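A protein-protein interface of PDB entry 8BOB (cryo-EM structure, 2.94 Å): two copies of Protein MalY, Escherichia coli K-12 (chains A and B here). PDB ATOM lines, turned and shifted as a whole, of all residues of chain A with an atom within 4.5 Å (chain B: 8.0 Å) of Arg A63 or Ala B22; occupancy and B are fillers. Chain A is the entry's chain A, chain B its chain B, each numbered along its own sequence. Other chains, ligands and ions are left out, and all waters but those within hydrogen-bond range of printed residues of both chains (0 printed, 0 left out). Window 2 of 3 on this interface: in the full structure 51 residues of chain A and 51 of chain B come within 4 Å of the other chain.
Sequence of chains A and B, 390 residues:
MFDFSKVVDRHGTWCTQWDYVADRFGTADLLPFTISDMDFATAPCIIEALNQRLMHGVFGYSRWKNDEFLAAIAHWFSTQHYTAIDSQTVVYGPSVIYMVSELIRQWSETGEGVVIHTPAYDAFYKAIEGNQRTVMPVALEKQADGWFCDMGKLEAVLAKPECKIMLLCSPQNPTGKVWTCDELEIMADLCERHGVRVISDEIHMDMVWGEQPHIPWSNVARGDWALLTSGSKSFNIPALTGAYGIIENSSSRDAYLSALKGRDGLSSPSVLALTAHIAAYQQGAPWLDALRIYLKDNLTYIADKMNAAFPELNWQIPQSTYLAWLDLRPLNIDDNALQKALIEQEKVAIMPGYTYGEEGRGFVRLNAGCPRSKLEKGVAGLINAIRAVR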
ATOM      1  N   SER A  62     -26.409  21.840  33.151  1.00  0.00           N
ATOM      2  CA  SER A  62     -26.200  23.045  32.374  1.00  0.00           C
ATOM      3  C   SER A  62     -25.659  22.657  31.014  1.00  0.00           C
ATOM      4  O   SER A  62     -25.260  21.516  30.788  1.00  0.00           O
ATOM      5  CB  SER A  62     -25.244  23.999  33.084  1.00  0.00           C
ATOM      6  OG  SER A  62     -25.924  24.691  34.109  1.00  0.00           O
ATOM      7  N   ARG A  63     -25.650  23.615  30.099  1.00  0.00           N
ATOM      8  CA  ARG A  63     -25.222  23.371  28.733  1.00  0.00           C
ATOM      9  C   ARG A  63     -24.088  24.314  28.368  1.00  0.00           C
ATOM     10  O   ARG A  63     -24.140  25.504  28.679  1.00  0.00           O
ATOM     11  CB  ARG A  63     -26.378  23.547  27.763  1.00  0.00           C
ATOM     12  CG  ARG A  63     -26.207  22.758  26.503  1.00  0.00           C
ATOM     13  CD  ARG A  63     -27.190  23.194  25.448  1.00  0.00           C
ATOM     14  NE  ARG A  63     -28.538  22.722  25.729  1.00  0.00           N
ATOM     15  CZ  ARG A  63     -28.987  21.520  25.387  1.00  0.00           C
ATOM     16  NH1 ARG A  63     -28.191  20.669  24.759  1.00  0.00           N
ATOM     17  NH2 ARG A  63     -30.229  21.167  25.676  1.00  0.00           N
ATOM     18  N   TRP A  64     -23.056  23.782  27.720  1.00  0.00           N
ATOM     19  CA  TRP A  64     -21.941  24.614  27.297  1.00  0.00           C
ATOM     20  C   TRP A  64     -22.118  25.178  25.899  1.00  0.00           C
ATOM     21  O   TRP A  64     -21.532  26.221  25.598  1.00  0.00           O
ATOM     22  CB  TRP A  64     -20.625  23.840  27.368  1.00  0.00           C
ATOM     23  CG  TRP A  64     -20.501  22.748  26.379  1.00  0.00           C
ATOM     24  CD1 TRP A  64     -20.711  21.431  26.604  1.00  0.00           C
ATOM     25  CD2 TRP A  64     -20.123  22.865  25.007  1.00  0.00           C
ATOM     26  NE1 TRP A  64     -20.497  20.714  25.460  1.00  0.00           N
ATOM     27  CE2 TRP A  64     -20.135  21.576  24.463  1.00  0.00           C
ATOM     28  CE3 TRP A  64     -19.778  23.937  24.186  1.00  0.00           C
ATOM     29  CZ2 TRP A  64     -19.818  21.327  23.141  1.00  0.00           C
ATOM     30  CZ3 TRP A  64     -19.472  23.688  22.881  1.00  0.00           C
ATOM     31  CH2 TRP A  64     -19.492  22.396  22.367  1.00  0.00           C
ATOM     32  N   LYS A  65     -22.922  24.536  25.047  1.00  0.00           N
ATOM     33  CA  LYS A  65     -23.197  25.048  23.708  1.00  0.00           C
ATOM     34  C   LYS A  65     -24.116  26.238  23.882  1.00  0.00           C
ATOM     35  O   LYS A  65     -25.236  26.280  23.368  1.00  0.00           O
ATOM     36  CB  LYS A  65     -23.832  23.980  22.824  1.00  0.00           C
ATOM     37  CG  LYS A  65     -23.909  24.317  21.343  1.00  0.00           C
ATOM     38  CD  LYS A  65     -22.570  24.680  20.772  1.00  0.00           C
ATOM     39  CE  LYS A  65     -22.564  24.450  19.279  1.00  0.00           C
ATOM     40  NZ  LYS A  65     -22.793  23.015  19.004  1.00  0.00           N
ATOM     41  N   ASN A  66     -23.619  27.200  24.629  1.00  0.00           N
ATOM     42  CA  ASN A  66     -24.361  28.347  25.099  1.00  0.00           C
ATOM     43  C   ASN A  66     -24.419  29.370  23.977  1.00  0.00           C
ATOM     44  O   ASN A  66     -24.151  29.066  22.813  1.00  0.00           O
ATOM     45  CB  ASN A  66     -23.669  28.889  26.338  1.00  0.00           C
ATOM     46  CG  ASN A  66     -24.614  29.292  27.414  1.00  0.00           C
ATOM     47  OD1 ASN A  66     -25.805  28.995  27.376  1.00  0.00           O
ATOM     48  ND2 ASN A  66     -24.081  29.980  28.400  1.00  0.00           N
ATOM     49  N   PRO A 269     -20.773  20.266  31.708  1.00  0.00           N
ATOM     50  CA  PRO A 269     -19.688  21.161  32.098  1.00  0.00           C
ATOM     51  C   PRO A 269     -19.818  21.578  33.551  1.00  0.00           C
ATOM     52  O   PRO A 269     -20.793  21.282  34.233  1.00  0.00           O
ATOM     53  CB  PRO A 269     -19.896  22.356  31.179  1.00  0.00           C
ATOM     54  CG  PRO A 269     -21.346  22.427  31.069  1.00  0.00           C
ATOM     55  CD  PRO A 269     -21.830  21.001  31.005  1.00  0.00           C
ATOM     56  N   LEU A 274     -17.721  27.953  33.398  1.00  0.00           N
ATOM     57  CA  LEU A 274     -18.254  28.800  32.342  1.00  0.00           C
ATOM     58  C   LEU A 274     -18.521  30.206  32.850  1.00  0.00           C
ATOM     59  O   LEU A 274     -18.232  31.184  32.156  1.00  0.00           O
ATOM     60  CB  LEU A 274     -19.526  28.192  31.768  1.00  0.00           C
ATOM     61  CG  LEU A 274     -19.463  26.733  31.346  1.00  0.00           C
ATOM     62  CD1 LEU A 274     -20.815  26.291  30.874  1.00  0.00           C
ATOM     63  CD2 LEU A 274     -18.444  26.543  30.266  1.00  0.00           C
ATOM     64  N   THR B  13     -30.547  30.289  33.011  1.00  0.00           N
ATOM     65  CA  THR B  13     -29.381  29.740  33.685  1.00  0.00           C
ATOM     66  C   THR B  13     -28.757  28.596  32.908  1.00  0.00           C
ATOM     67  O   THR B  13     -28.027  27.794  33.497  1.00  0.00           O
ATOM     68  CB  THR B  13     -29.742  29.258  35.088  1.00  0.00           C
ATOM     69  OG1 THR B  13     -30.929  28.468  35.019  1.00  0.00           O
ATOM     70  CG2 THR B  13     -29.977  30.421  36.012  1.00  0.00           C
ATOM     71  N   TRP B  14     -29.047  28.485  31.615  1.00  0.00           N
ATOM     72  CA  TRP B  14     -28.422  27.520  30.723  1.00  0.00           C
ATOM     73  C   TRP B  14     -28.817  26.094  31.055  1.00  0.00           C
ATOM     74  O   TRP B  14     -28.181  25.157  30.582  1.00  0.00           O
ATOM     75  CB  TRP B  14     -26.900  27.650  30.769  1.00  0.00           C
ATOM     76  CG  TRP B  14     -26.467  29.029  30.528  1.00  0.00           C
ATOM     77  CD1 TRP B  14     -27.116  29.967  29.805  1.00  0.00           C
ATOM     78  CD2 TRP B  14     -25.391  29.699  31.174  1.00  0.00           C
ATOM     79  NE1 TRP B  14     -26.460  31.157  29.871  1.00  0.00           N
ATOM     80  CE2 TRP B  14     -25.407  31.027  30.730  1.00  0.00           C
ATOM     81  CE3 TRP B  14     -24.397  29.297  32.059  1.00  0.00           C
ATOM     82  CZ2 TRP B  14     -24.462  31.949  31.124  1.00  0.00           C
ATOM     83  CZ3 TRP B  14     -23.466  30.213  32.456  1.00  0.00           C
ATOM     84  CH2 TRP B  14     -23.499  31.522  31.991  1.00  0.00           C
ATOM     85  N   CYS B  15     -29.855  25.905  31.864  1.00  0.00           N
ATOM     86  CA  CYS B  15     -30.213  24.574  32.323  1.00  0.00           C
ATOM     87  C   CYS B  15     -30.935  23.812  31.227  1.00  0.00           C
ATOM     88  O   CYS B  15     -31.815  24.348  30.556  1.00  0.00           O
ATOM     89  CB  CYS B  15     -31.084  24.648  33.574  1.00  0.00           C
ATOM     90  SG  CYS B  15     -32.658  25.456  33.355  1.00  0.00           S
ATOM     91  N   THR B  16     -30.562  22.548  31.054  1.00  0.00           N
ATOM     92  CA  THR B  16     -31.085  21.782  29.937  1.00  0.00           C
ATOM     93  C   THR B  16     -32.580  21.517  30.040  1.00  0.00           C
ATOM     94  O   THR B  16     -33.177  21.082  29.052  1.00  0.00           O
ATOM     95  CB  THR B  16     -30.335  20.462  29.814  1.00  0.00           C
ATOM     96  OG1 THR B  16     -30.357  19.782  31.068  1.00  0.00           O
ATOM     97  CG2 THR B  16     -28.902  20.713  29.433  1.00  0.00           C
ATOM     98  N   GLN B  17     -33.205  21.776  31.183  1.00  0.00           N
ATOM     99  CA  GLN B  17     -34.630  21.497  31.298  1.00  0.00           C
ATOM    100  C   GLN B  17     -35.491  22.705  30.960  1.00  0.00           C
ATOM    101  O   GLN B  17     -36.425  22.598  30.164  1.00  0.00           O
ATOM    102  CB  GLN B  17     -34.967  21.008  32.703  1.00  0.00           C
ATOM    103  CG  GLN B  17     -36.132  20.056  32.706  1.00  0.00           C
ATOM    104  CD  GLN B  17     -36.352  19.418  34.044  1.00  0.00           C
ATOM    105  OE1 GLN B  17     -36.376  20.094  35.066  1.00  0.00           O
ATOM    106  NE2 GLN B  17     -36.493  18.103  34.052  1.00  0.00           N
ATOM    107  N   ASP B  19     -34.481  25.788  29.709  1.00  0.00           N
ATOM    108  CA  ASP B  19     -34.012  26.767  28.741  1.00  0.00           C
ATOM    109  C   ASP B  19     -33.871  26.211  27.340  1.00  0.00           C
ATOM    110  O   ASP B  19     -33.567  26.967  26.415  1.00  0.00           O
ATOM    111  CB  ASP B  19     -32.672  27.350  29.183  1.00  0.00           C
ATOM    112  CG  ASP B  19     -32.816  28.329  30.314  1.00  0.00           C
ATOM    113  OD1 ASP B  19     -33.929  28.446  30.856  1.00  0.00           O
ATOM    114  OD2 ASP B  19     -31.821  28.989  30.664  1.00  0.00           O
ATOM    115  N   TYR B  20     -34.078  24.919  27.150  1.00  0.00           N
ATOM    116  CA  TYR B  20     -33.810  24.284  25.869  1.00  0.00           C
ATOM    117  C   TYR B  20     -34.974  23.389  25.474  1.00  0.00           C
ATOM    118  O   TYR B  20     -35.186  22.334  26.080  1.00  0.00           O
ATOM    119  CB  TYR B  20     -32.508  23.490  25.939  1.00  0.00           C
ATOM    120  CG  TYR B  20     -31.315  24.377  26.170  1.00  0.00           C
ATOM    121  CD1 TYR B  20     -30.686  25.004  25.113  1.00  0.00           C
ATOM    122  CD2 TYR B  20     -30.835  24.608  27.441  1.00  0.00           C
ATOM    123  CE1 TYR B  20     -29.608  25.826  25.318  1.00  0.00           C
ATOM    124  CE2 TYR B  20     -29.755  25.427  27.652  1.00  0.00           C
ATOM    125  CZ  TYR B  20     -29.147  26.032  26.588  1.00  0.00           C
ATOM    126  OH  TYR B  20     -28.068  26.852  26.790  1.00  0.00           O
ATOM    127  N   VAL B  21     -35.722  23.809  24.454  1.00  0.00           N
ATOM    128  CA  VAL B  21     -36.804  22.976  23.940  1.00  0.00           C
ATOM    129  C   VAL B  21     -36.253  21.703  23.302  1.00  0.00           C
ATOM    130  O   VAL B  21     -36.666  20.590  23.649  1.00  0.00           O
ATOM    131  CB  VAL B  21     -37.687  23.781  22.967  1.00  0.00           C
ATOM    132  CG1 VAL B  21     -36.903  24.303  21.776  1.00  0.00           C
ATOM    133  CG2 VAL B  21     -38.807  22.915  22.481  1.00  0.00           C
ATOM    134  N   ALA B  22     -35.305  21.840  22.383  1.00  0.00           N
ATOM    135  CA  ALA B  22     -34.733  20.705  21.685  1.00  0.00           C
ATOM    136  C   ALA B  22     -33.881  19.908  22.657  1.00  0.00           C
ATOM    137  O   ALA B  22     -33.100  20.473  23.426  1.00  0.00           O
ATOM    138  CB  ALA B  22     -33.883  21.148  20.482  1.00  0.00           C
ATOM    139  N   ASP B  23     -34.050  18.593  22.629  1.00  0.00           N
ATOM    140  CA  ASP B  23     -35.062  17.957  21.797  1.00  0.00           C
ATOM    141  C   ASP B  23     -36.177  17.393  22.663  1.00  0.00           C
ATOM    142  O   ASP B  23     -36.868  16.456  22.270  1.00  0.00           O
ATOM    143  CB  ASP B  23     -34.444  16.868  20.946  1.00  0.00           C
ATOM    144  N   ARG B  24     -36.340  17.971  23.855  1.00  0.00           N
ATOM    145  CA  ARG B  24     -37.372  17.499  24.774  1.00  0.00           C
ATOM    146  C   ARG B  24     -38.762  17.703  24.193  1.00  0.00           C
ATOM    147  O   ARG B  24     -39.706  16.986  24.545  1.00  0.00           O
ATOM    148  CB  ARG B  24     -37.243  18.217  26.114  1.00  0.00           C
ATOM    149  N   PHE B  25     -38.903  18.678  23.303  1.00  0.00           N
ATOM    150  CA  PHE B  25     -40.182  19.036  22.716  1.00  0.00           C
ATOM    151  C   PHE B  25     -39.908  19.859  21.471  1.00  0.00           C
ATOM    152  O   PHE B  25     -38.792  19.885  20.952  1.00  0.00           O
ATOM    153  CB  PHE B  25     -41.053  19.812  23.699  1.00  0.00           C
ATOM    154  N   GLY B  26     -40.951  20.522  20.990  1.00  0.00           N
ATOM    155  CA  GLY B  26     -40.812  21.491  19.917  1.00  0.00           C
ATOM    156  C   GLY B  26     -41.531  22.799  20.209  1.00  0.00           C
ATOM    157  O   GLY B  26     -41.256  23.801  19.545  1.00  0.00           O
ATOM    158  N   THR B  27     -42.435  22.821  21.188  1.00  0.00           N
ATOM    159  CA  THR B  27     -43.250  24.011  21.406  1.00  0.00           C
ATOM    160  C   THR B  27     -42.522  25.045  22.254  1.00  0.00           C
ATOM    161  O   THR B  27     -42.841  26.237  22.194  1.00  0.00           O
ATOM    162  CB  THR B  27     -44.579  23.625  22.051  1.00  0.00           C
ATOM    163  N   ALA B  28     -41.565  24.606  23.073  1.00  0.00           N
ATOM    164  CA  ALA B  28     -40.739  25.494  23.895  1.00  0.00           C
ATOM    165  C   ALA B  28     -41.550  26.249  24.943  1.00  0.00           C
ATOM    166  O   ALA B  28     -41.012  27.088  25.666  1.00  0.00           O
ATOM    167  CB  ALA B  28     -39.949  26.480  23.033  1.00  0.00           C
ATOM    168  N   ILE B  35     -35.892  15.827  32.250  1.00  0.00           N
ATOM    169  CA  ILE B  35     -34.524  15.629  32.710  1.00  0.00           C
ATOM    170  C   ILE B  35     -34.511  15.391  34.210  1.00  0.00           C
ATOM    171  O   ILE B  35     -35.284  15.979  34.969  1.00  0.00           O
ATOM    172  CB  ILE B  35     -33.654  16.830  32.301  1.00  0.00           C
ATOM    173  CG1 ILE B  35     -33.608  16.899  30.784  1.00  0.00           C
ATOM    174  CG2 ILE B  35     -32.261  16.693  32.847  1.00  0.00           C
ATOM    175  CD1 ILE B  35     -33.134  18.191  30.266  1.00  0.00           C
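The backbone NH (N) of Thr B13 lies within hydrogen-bond range of the side-chain carboxylate (OD2) of Asp B19 (3.0 Å).
The side-chain carboxylate of Asp B19 is in hydrogen-bond range of the backbone NH of Trp B14, at 3.0 Å.
Printed residues of chain B that touch a printed residue of chain A: Thr B13, Trp B14, Thr B16, Tyr B20 and Ala B22.
Among the printed residues, 8 pairs touch across the chains.
Printed residues of chain B within 4 Å of Arg A63: Trp B14 (3.0 Å), Tyr B20 (3.2 Å) and Ala B22 (3.7 Å).
Ala B22 touches just one residue of chain A: Arg A63.
Printed residues of chain B within 4 Å of Ser A62: Thr B13, Trp B14 and Thr B16.
Of the printed residues of chain B, Asn A66 touches Trp B14 (2.9 Å) and Tyr B20 (3.2 Å).
Printed residues of chain A within 4 Å of Thr B16: Ser A62.
Asp B23 touches none of the printed residues of chain A.
Among the printed residues, pairs that only touch across the chains: Ser A62 with Thr B13 (3.8 Å), Ser A62 with Trp B14 (3.4 Å), Ser A62 with Thr B16 (3.97 Å), Arg A63 with Tyr B20 (3.2 Å) and Arg A63 with Ala B22 (3.7 Å).
The backbone carbonyl oxygen (O) of Trp B14 lies within hydrogen-bond range of the backbone NH (N) of Arg A63, 3.0 Å away.
ND2 of Asn A66 lies close to NE1 of Trp B14 (3.0 Å).
OD1 of Asn A66 is in hydrogen-bond range of OH of Tyr B20, 3.2 Å away.
No position is printed for both chains.
Of the 8 pairs that touch across the chains among the printed residues, none has its exchanged pair printed and touching as well.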
